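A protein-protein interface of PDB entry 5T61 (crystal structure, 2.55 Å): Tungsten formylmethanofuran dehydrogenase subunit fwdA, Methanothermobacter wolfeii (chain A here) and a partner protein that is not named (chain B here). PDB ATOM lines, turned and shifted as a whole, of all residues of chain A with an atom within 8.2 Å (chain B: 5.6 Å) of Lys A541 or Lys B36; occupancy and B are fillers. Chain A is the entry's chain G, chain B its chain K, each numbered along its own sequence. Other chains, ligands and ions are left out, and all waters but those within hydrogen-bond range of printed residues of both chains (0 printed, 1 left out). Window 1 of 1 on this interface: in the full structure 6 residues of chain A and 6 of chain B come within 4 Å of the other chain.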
ATOM      1  N   GLU A 341      17.364   4.434 -32.047  1.00  0.00           N
ATOM      2  CA  GLU A 341      18.165   4.279 -30.838  1.00  0.00           C
ATOM      3  C   GLU A 341      18.042   2.887 -30.226  1.00  0.00           C
ATOM      4  O   GLU A 341      16.940   2.350 -30.076  1.00  0.00           O
ATOM      5  CB  GLU A 341      17.748   5.348 -29.829  1.00  0.00           C
ATOM      6  CG  GLU A 341      16.269   5.317 -29.480  1.00  0.00           C
ATOM      7  CD  GLU A 341      15.741   6.667 -29.054  1.00  0.00           C
ATOM      8  OE1 GLU A 341      15.721   7.588 -29.899  1.00  0.00           O
ATOM      9  OE2 GLU A 341      15.345   6.810 -27.879  1.00  0.00           O
ATOM     10  N   ALA A 534      13.316  -4.649 -14.470  1.00  0.00           N
ATOM     11  CA  ALA A 534      14.007  -3.622 -13.701  1.00  0.00           C
ATOM     12  C   ALA A 534      15.213  -3.100 -14.472  1.00  0.00           C
ATOM     13  O   ALA A 534      15.469  -1.890 -14.492  1.00  0.00           O
ATOM     14  CB  ALA A 534      14.427  -4.169 -12.337  1.00  0.00           C
ATOM     15  N   ASN A 535      15.955  -3.996 -15.129  1.00  0.00           N
ATOM     16  CA  ASN A 535      17.089  -3.559 -15.935  1.00  0.00           C
ATOM     17  C   ASN A 535      16.639  -2.737 -17.137  1.00  0.00           C
ATOM     18  O   ASN A 535      17.251  -1.711 -17.457  1.00  0.00           O
ATOM     19  CB  ASN A 535      17.906  -4.761 -16.404  1.00  0.00           C
ATOM     20  CG  ASN A 535      19.048  -4.358 -17.315  1.00  0.00           C
ATOM     21  OD1 ASN A 535      19.804  -3.437 -17.005  1.00  0.00           O
ATOM     22  ND2 ASN A 535      19.165  -5.028 -18.457  1.00  0.00           N
ATOM     23  N   VAL A 536      15.573  -3.169 -17.816  1.00  0.00           N
ATOM     24  CA  VAL A 536      15.092  -2.438 -18.986  1.00  0.00           C
ATOM     25  C   VAL A 536      14.669  -1.030 -18.590  1.00  0.00           C
ATOM     26  O   VAL A 536      15.031  -0.046 -19.246  1.00  0.00           O
ATOM     27  CB  VAL A 536      13.945  -3.206 -19.670  1.00  0.00           C
ATOM     28  CG1 VAL A 536      13.258  -2.325 -20.699  1.00  0.00           C
ATOM     29  CG2 VAL A 536      14.466  -4.476 -20.327  1.00  0.00           C
ATOM     30  N   GLU A 537      13.897  -0.910 -17.509  1.00  0.00           N
ATOM     31  CA  GLU A 537      13.453   0.411 -17.079  1.00  0.00           C
ATOM     32  C   GLU A 537      14.626   1.298 -16.666  1.00  0.00           C
ATOM     33  O   GLU A 537      14.533   2.527 -16.761  1.00  0.00           O
ATOM     34  CB  GLU A 537      12.431   0.289 -15.946  1.00  0.00           C
ATOM     35  CG  GLU A 537      11.752   1.611 -15.616  1.00  0.00           C
ATOM     36  CD  GLU A 537      10.493   1.450 -14.786  1.00  0.00           C
ATOM     37  OE1 GLU A 537       9.859   2.479 -14.473  1.00  0.00           O
ATOM     38  OE2 GLU A 537      10.127   0.300 -14.462  1.00  0.00           O
ATOM     39  N   SER A 538      15.731   0.706 -16.205  1.00  0.00           N
ATOM     40  CA  SER A 538      16.903   1.515 -15.869  1.00  0.00           C
ATOM     41  C   SER A 538      17.544   2.115 -17.116  1.00  0.00           C
ATOM     42  O   SER A 538      17.925   3.291 -17.117  1.00  0.00           O
ATOM     43  CB  SER A 538      17.924   0.685 -15.090  1.00  0.00           C
ATOM     44  OG  SER A 538      17.521   0.505 -13.744  1.00  0.00           O
ATOM     45  N   LYS A 539      17.679   1.327 -18.187  1.00  0.00           N
ATOM     46  CA  LYS A 539      18.295   1.863 -19.396  1.00  0.00           C
ATOM     47  C   LYS A 539      17.394   2.880 -20.087  1.00  0.00           C
ATOM     48  O   LYS A 539      17.897   3.811 -20.728  1.00  0.00           O
ATOM     49  CB  LYS A 539      18.674   0.735 -20.359  1.00  0.00           C
ATOM     50  CG  LYS A 539      19.833  -0.132 -19.875  1.00  0.00           C
ATOM     51  CD  LYS A 539      20.899  -0.320 -20.956  1.00  0.00           C
ATOM     52  CE  LYS A 539      20.298  -0.793 -22.270  1.00  0.00           C
ATOM     53  NZ  LYS A 539      21.310  -1.374 -23.192  1.00  0.00           N
ATOM     54  N   PHE A 540      16.072   2.735 -19.962  1.00  0.00           N
ATOM     55  CA  PHE A 540      15.172   3.746 -20.506  1.00  0.00           C
ATOM     56  C   PHE A 540      15.405   5.096 -19.839  1.00  0.00           C
ATOM     57  O   PHE A 540      15.475   6.132 -20.512  1.00  0.00           O
ATOM     58  CB  PHE A 540      13.713   3.313 -20.340  1.00  0.00           C
ATOM     59  CG  PHE A 540      13.148   2.608 -21.543  1.00  0.00           C
ATOM     60  CD1 PHE A 540      13.340   1.247 -21.725  1.00  0.00           C
ATOM     61  CD2 PHE A 540      12.448   3.316 -22.504  1.00  0.00           C
ATOM     62  CE1 PHE A 540      12.820   0.603 -22.835  1.00  0.00           C
ATOM     63  CE2 PHE A 540      11.933   2.681 -23.616  1.00  0.00           C
ATOM     64  CZ  PHE A 540      12.118   1.324 -23.782  1.00  0.00           C
ATOM     65  N   LYS A 541      15.527   5.105 -18.507  1.00  0.00           N
ATOM     66  CA  LYS A 541      15.778   6.354 -17.793  1.00  0.00           C
ATOM     67  C   LYS A 541      17.106   6.973 -18.212  1.00  0.00           C
ATOM     68  O   LYS A 541      17.210   8.195 -18.368  1.00  0.00           O
ATOM     69  CB  LYS A 541      15.755   6.121 -16.280  1.00  0.00           C
ATOM     70  CG  LYS A 541      14.387   5.775 -15.707  1.00  0.00           C
ATOM     71  CD  LYS A 541      14.453   5.594 -14.196  1.00  0.00           C
ATOM     72  CE  LYS A 541      13.211   4.900 -13.662  1.00  0.00           C
ATOM     73  NZ  LYS A 541      13.441   4.309 -12.313  1.00  0.00           N
ATOM     74  N   GLN A 542      18.135   6.144 -18.385  1.00  0.00           N
ATOM     75  CA  GLN A 542      19.461   6.627 -18.762  1.00  0.00           C
ATOM     76  C   GLN A 542      19.557   6.956 -20.249  1.00  0.00           C
ATOM     77  O   GLN A 542      19.996   8.049 -20.622  1.00  0.00           O
ATOM     78  CB  GLN A 542      20.516   5.582 -18.385  1.00  0.00           C
ATOM     79  CG  GLN A 542      20.613   5.247 -16.913  1.00  0.00           C
ATOM     80  CD  GLN A 542      21.532   4.070 -16.651  1.00  0.00           C
ATOM     81  OE1 GLN A 542      21.153   2.916 -16.877  1.00  0.00           O
ATOM     82  NE2 GLN A 542      22.771   4.353 -16.267  1.00  0.00           N
ATOM     83  N   TYR A 543      19.169   6.018 -21.118  1.00  0.00           N
ATOM     84  CA  TYR A 543      19.651   6.026 -22.491  1.00  0.00           C
ATOM     85  C   TYR A 543      18.582   6.181 -23.565  1.00  0.00           C
ATOM     86  O   TYR A 543      18.916   6.611 -24.674  1.00  0.00           O
ATOM     87  CB  TYR A 543      20.453   4.745 -22.766  1.00  0.00           C
ATOM     88  CG  TYR A 543      21.623   4.583 -21.820  1.00  0.00           C
ATOM     89  CD1 TYR A 543      22.496   5.636 -21.581  1.00  0.00           C
ATOM     90  CD2 TYR A 543      21.852   3.381 -21.162  1.00  0.00           C
ATOM     91  CE1 TYR A 543      23.565   5.499 -20.717  1.00  0.00           C
ATOM     92  CE2 TYR A 543      22.921   3.234 -20.295  1.00  0.00           C
ATOM     93  CZ  TYR A 543      23.776   4.296 -20.078  1.00  0.00           C
ATOM     94  OH  TYR A 543      24.842   4.154 -19.216  1.00  0.00           O
ATOM     95  N   TYR A 544      17.324   5.850 -23.286  1.00  0.00           N
ATOM     96  CA  TYR A 544      16.279   6.103 -24.266  1.00  0.00           C
ATOM     97  C   TYR A 544      15.881   7.575 -24.263  1.00  0.00           C
ATOM     98  O   TYR A 544      16.162   8.324 -23.325  1.00  0.00           O
ATOM     99  CB  TYR A 544      15.050   5.235 -23.995  1.00  0.00           C
ATOM    100  CG  TYR A 544      14.993   3.948 -24.798  1.00  0.00           C
ATOM    101  CD1 TYR A 544      14.432   3.924 -26.070  1.00  0.00           C
ATOM    102  CD2 TYR A 544      15.479   2.756 -24.275  1.00  0.00           C
ATOM    103  CE1 TYR A 544      14.368   2.750 -26.804  1.00  0.00           C
ATOM    104  CE2 TYR A 544      15.417   1.579 -24.999  1.00  0.00           C
ATOM    105  CZ  TYR A 544      14.860   1.581 -26.262  1.00  0.00           C
ATOM    106  OH  TYR A 544      14.802   0.408 -26.978  1.00  0.00           O
ATOM    107  N   SER A 545      15.211   7.985 -25.337  1.00  0.00           N
ATOM    108  CA  SER A 545      14.726   9.352 -25.474  1.00  0.00           C
ATOM    109  C   SER A 545      13.235   9.481 -25.181  1.00  0.00           C
ATOM    110  O   SER A 545      12.680  10.572 -25.336  1.00  0.00           O
ATOM    111  CB  SER A 545      15.037   9.883 -26.879  1.00  0.00           C
ATOM    112  OG  SER A 545      14.211   9.262 -27.850  1.00  0.00           O
ATOM    113  N   VAL A 546      12.581   8.401 -24.761  1.00  0.00           N
ATOM    114  CA  VAL A 546      11.205   8.441 -24.290  1.00  0.00           C
ATOM    115  C   VAL A 546      11.183   7.834 -22.892  1.00  0.00           C
ATOM    116  O   VAL A 546      12.179   7.297 -22.407  1.00  0.00           O
ATOM    117  CB  VAL A 546      10.224   7.697 -25.223  1.00  0.00           C
ATOM    118  CG1 VAL A 546      10.264   8.280 -26.637  1.00  0.00           C
ATOM    119  CG2 VAL A 546      10.503   6.201 -25.219  1.00  0.00           C
ATOM    120  N   ASN A 547      10.025   7.917 -22.248  1.00  0.00           N
ATOM    121  CA  ASN A 547       9.855   7.387 -20.905  1.00  0.00           C
ATOM    122  C   ASN A 547       9.272   5.981 -20.964  1.00  0.00           C
ATOM    123  O   ASN A 547       8.423   5.685 -21.809  1.00  0.00           O
ATOM    124  CB  ASN A 547       8.961   8.302 -20.070  1.00  0.00           C
ATOM    125  CG  ASN A 547       9.703   9.520 -19.553  1.00  0.00           C
ATOM    126  OD1 ASN A 547      10.747   9.897 -20.089  1.00  0.00           O
ATOM    127  ND2 ASN A 547       9.178  10.134 -18.500  1.00  0.00           N
ATOM    128  N   PHE A 548       9.763   5.113 -20.071  1.00  0.00           N
ATOM    129  CA  PHE A 548       9.372   3.703 -20.063  1.00  0.00           C
ATOM    130  C   PHE A 548       7.858   3.516 -20.113  1.00  0.00           C
ATOM    131  O   PHE A 548       7.358   2.612 -20.793  1.00  0.00           O
ATOM    132  CB  PHE A 548       9.959   3.018 -18.827  1.00  0.00           C
ATOM    133  CG  PHE A 548       9.642   1.549 -18.732  1.00  0.00           C
ATOM    134  CD1 PHE A 548      10.288   0.630 -19.541  1.00  0.00           C
ATOM    135  CD2 PHE A 548       8.714   1.088 -17.811  1.00  0.00           C
ATOM    136  CE1 PHE A 548       9.997  -0.721 -19.449  1.00  0.00           C
ATOM    137  CE2 PHE A 548       8.422  -0.261 -17.712  1.00  0.00           C
ATOM    138  CZ  PHE A 548       9.064  -1.166 -18.530  1.00  0.00           C
ATOM    139  N   ALA A 549       7.111   4.355 -19.392  1.00  0.00           N
ATOM    140  CA  ALA A 549       5.662   4.182 -19.316  1.00  0.00           C
ATOM    141  C   ALA A 549       4.978   4.386 -20.664  1.00  0.00           C
ATOM    142  O   ALA A 549       3.915   3.806 -20.913  1.00  0.00           O
ATOM    143  CB  ALA A 549       5.074   5.138 -18.280  1.00  0.00           C
ATOM    144  N   ILE B  20      20.075  19.913 -16.178  1.00  0.00           N
ATOM    145  CA  ILE B  20      20.778  18.744 -16.696  1.00  0.00           C
ATOM    146  C   ILE B  20      22.282  18.881 -16.489  1.00  0.00           C
ATOM    147  O   ILE B  20      22.964  17.907 -16.155  1.00  0.00           O
ATOM    148  CB  ILE B  20      20.428  18.519 -18.180  1.00  0.00           C
ATOM    149  CG1 ILE B  20      18.910  18.424 -18.371  1.00  0.00           C
ATOM    150  CG2 ILE B  20      21.139  17.287 -18.720  1.00  0.00           C
ATOM    151  CD1 ILE B  20      18.244  17.391 -17.483  1.00  0.00           C
ATOM    152  N   PRO B  30      19.307   9.685 -12.319  1.00  0.00           N
ATOM    153  CA  PRO B  30      19.723   9.203 -13.649  1.00  0.00           C
ATOM    154  C   PRO B  30      18.912   9.782 -14.799  1.00  0.00           C
ATOM    155  O   PRO B  30      19.451   9.930 -15.903  1.00  0.00           O
ATOM    156  CB  PRO B  30      19.557   7.682 -13.547  1.00  0.00           C
ATOM    157  CG  PRO B  30      19.582   7.375 -12.099  1.00  0.00           C
ATOM    158  CD  PRO B  30      19.109   8.589 -11.355  1.00  0.00           C
ATOM    159  N   GLU B  31      17.632  10.096 -14.591  1.00  0.00           N
ATOM    160  CA  GLU B  31      16.854  10.730 -15.652  1.00  0.00           C
ATOM    161  C   GLU B  31      17.387  12.125 -15.963  1.00  0.00           C
ATOM    162  O   GLU B  31      17.457  12.527 -17.133  1.00  0.00           O
ATOM    163  CB  GLU B  31      15.379  10.779 -15.261  1.00  0.00           C
ATOM    164  CG  GLU B  31      14.798   9.447 -14.788  1.00  0.00           C
ATOM    165  CD  GLU B  31      13.384   9.589 -14.249  1.00  0.00           C
ATOM    166  OE1 GLU B  31      13.199  10.251 -13.206  1.00  0.00           O
ATOM    167  OE2 GLU B  31      12.451   9.053 -14.884  1.00  0.00           O
ATOM    168  N   VAL B  32      17.761  12.882 -14.928  1.00  0.00           N
ATOM    169  CA  VAL B  32      18.350  14.201 -15.146  1.00  0.00           C
ATOM    170  C   VAL B  32      19.729  14.075 -15.783  1.00  0.00           C
ATOM    171  O   VAL B  32      20.077  14.838 -16.691  1.00  0.00           O
ATOM    172  CB  VAL B  32      18.399  14.993 -13.826  1.00  0.00           C
ATOM    173  CG1 VAL B  32      19.280  16.226 -13.976  1.00  0.00           C
ATOM    174  CG2 VAL B  32      17.000  15.403 -13.411  1.00  0.00           C
ATOM    175  N   ALA B  33      20.537  13.117 -15.316  1.00  0.00           N
ATOM    176  CA  ALA B  33      21.837  12.876 -15.934  1.00  0.00           C
ATOM    177  C   ALA B  33      21.691  12.593 -17.424  1.00  0.00           C
ATOM    178  O   ALA B  33      22.539  12.996 -18.229  1.00  0.00           O
ATOM    179  CB  ALA B  33      22.551  11.724 -15.229  1.00  0.00           C
ATOM    180  N   GLY B  34      20.619  11.906 -17.805  1.00  0.00           N
ATOM    181  CA  GLY B  34      20.354  11.610 -19.197  1.00  0.00           C
ATOM    182  C   GLY B  34      19.500  12.657 -19.884  1.00  0.00           C
ATOM    183  O   GLY B  34      18.910  12.386 -20.930  1.00  0.00           O
ATOM    184  N   GLY B  35      19.380  13.843 -19.300  1.00  0.00           N
ATOM    185  CA  GLY B  35      18.740  14.942 -19.990  1.00  0.00           C
ATOM    186  C   GLY B  35      17.241  15.058 -19.825  1.00  0.00           C
ATOM    187  O   GLY B  35      16.640  15.962 -20.421  1.00  0.00           O
ATOM    188  N   LYS B  36      16.613  14.188 -19.044  1.00  0.00           N
ATOM    189  CA  LYS B  36      15.177  14.260 -18.828  1.00  0.00           C
ATOM    190  C   LYS B  36      14.866  15.024 -17.550  1.00  0.00           C
ATOM    191  O   LYS B  36      15.681  15.083 -16.625  1.00  0.00           O
ATOM    192  CB  LYS B  36      14.559  12.863 -18.749  1.00  0.00           C
ATOM    193  CG  LYS B  36      14.684  12.054 -20.025  1.00  0.00           C
ATOM    194  CD  LYS B  36      14.557  10.566 -19.738  1.00  0.00           C
ATOM    195  CE  LYS B  36      14.320   9.790 -21.021  1.00  0.00           C
ATOM    196  NZ  LYS B  36      13.885   8.389 -20.765  1.00  0.00           N
ATOM    197  N   GLY B  37      13.677  15.620 -17.509  1.00  0.00           N
ATOM    198  CA  GLY B  37      13.130  16.111 -16.269  1.00  0.00           C
ATOM    199  C   GLY B  37      12.837  14.937 -15.361  1.00  0.00           C
ATOM    200  O   GLY B  37      12.537  13.831 -15.822  1.00  0.00           O
ATOM    201  N   PRO B  38      12.940  15.142 -14.049  1.00  0.00           N
ATOM    202  CA  PRO B  38      12.688  14.035 -13.112  1.00  0.00           C
ATOM    203  C   PRO B  38      11.223  13.622 -13.125  1.00  0.00           C
ATOM    204  O   PRO B  38      10.324  14.465 -13.084  1.00  0.00           O
ATOM    205  CB  PRO B  38      13.103  14.615 -11.754  1.00  0.00           C
ATOM    206  CG  PRO B  38      13.037  16.096 -11.928  1.00  0.00           C
ATOM    207  CD  PRO B  38      13.357  16.378 -13.362  1.00  0.00           C
ATOM    208  N   ASP B  40      10.548  10.250 -11.248  1.00  0.00           N
ATOM    209  CA  ASP B  40      10.710   9.781  -9.882  1.00  0.00           C
ATOM    210  C   ASP B  40      10.865  10.965  -8.940  1.00  0.00           C
ATOM    211  O   ASP B  40      11.381  12.019  -9.325  1.00  0.00           O
ATOM    212  CB  ASP B  40      11.940   8.883  -9.797  1.00  0.00           C
ATOM    213  CG  ASP B  40      11.826   7.649 -10.662  1.00  0.00           C
ATOM    214  OD1 ASP B  40      10.685   7.298 -11.029  1.00  0.00           O
ATOM    215  OD2 ASP B  40      12.872   7.050 -11.000  1.00  0.00           O
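Among the printed residues, pairs that only touch across the chains: Lys A541 with Pro B30, Lys A541 with Glu B31, Lys A541 with Lys B36, Gln A542 with Gly B34 and Asn A547 with Lys B36.
The backbone carbonyl oxygen (O) of Phe A540 is in hydrogen-bond range of the side-chain amino group (NZ) of Lys B36, 2.8 Å away. NZ of Lys A541 lies within salt-bridge range of OD2 of Asp B40. The backbone carbonyl oxygen of Tyr A544 sits close to the side-chain amino group of Lys B36, at 3.4 Å. NZ of Lys B36 is in hydrogen-bond range of O of Val A546 (2.6 Å).
OE1 of Gln A542 lies close to O of Ser A538 (3.3 Å). The backbone NH (N) of Tyr A544 lies within hydrogen-bond range of the backbone carbonyl oxygen (O) of Lys A539, 3.3 Å away. The backbone NH (N) of Lys B36 is in hydrogen-bond range of the backbone carbonyl oxygen (O) of Glu B31 (2.7 Å). OE1 of Glu B31 lies within hydrogen-bond range of N of Asp B40 (3.3 Å).
Of the 17 printed residues of chain A, 6 touch a printed residue of chain B. Among the printed residues, Asp or Glu carboxylates within 4 Å of a Lys or Arg side-chain nitrogen of the other chain: Lys A541 with Asp B40 (3.1 Å).
Ala A534 touches none of the printed residues of chain B. Glu A537 touches none of the printed residues of chain B. Of the printed residues of chain B, Phe A540 touches Lys B36 (2.8 Å). Lys A541 touches just these residues of chain B: Pro B30, Glu B31, Lys B36 and Asp B40. Of the printed residues of chain B, Gln A542 touches Gly B34. Printed residues of chain B within 4 Å of Tyr A544: Lys B36 (3.3 Å). Lys B36 touches just these residues of chain A: Phe A540, Lys A541, Tyr A544, Val A546 and Asn A547. Of the printed residues of chain A, Asp B40 touches Lys A541. The nearest residue of chain B that does not touch Lys A541 is Gly B34 (4.7 Å). The nearest residue of chain A that does not touch Lys B36 is Ser A545 (4.3 Å).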
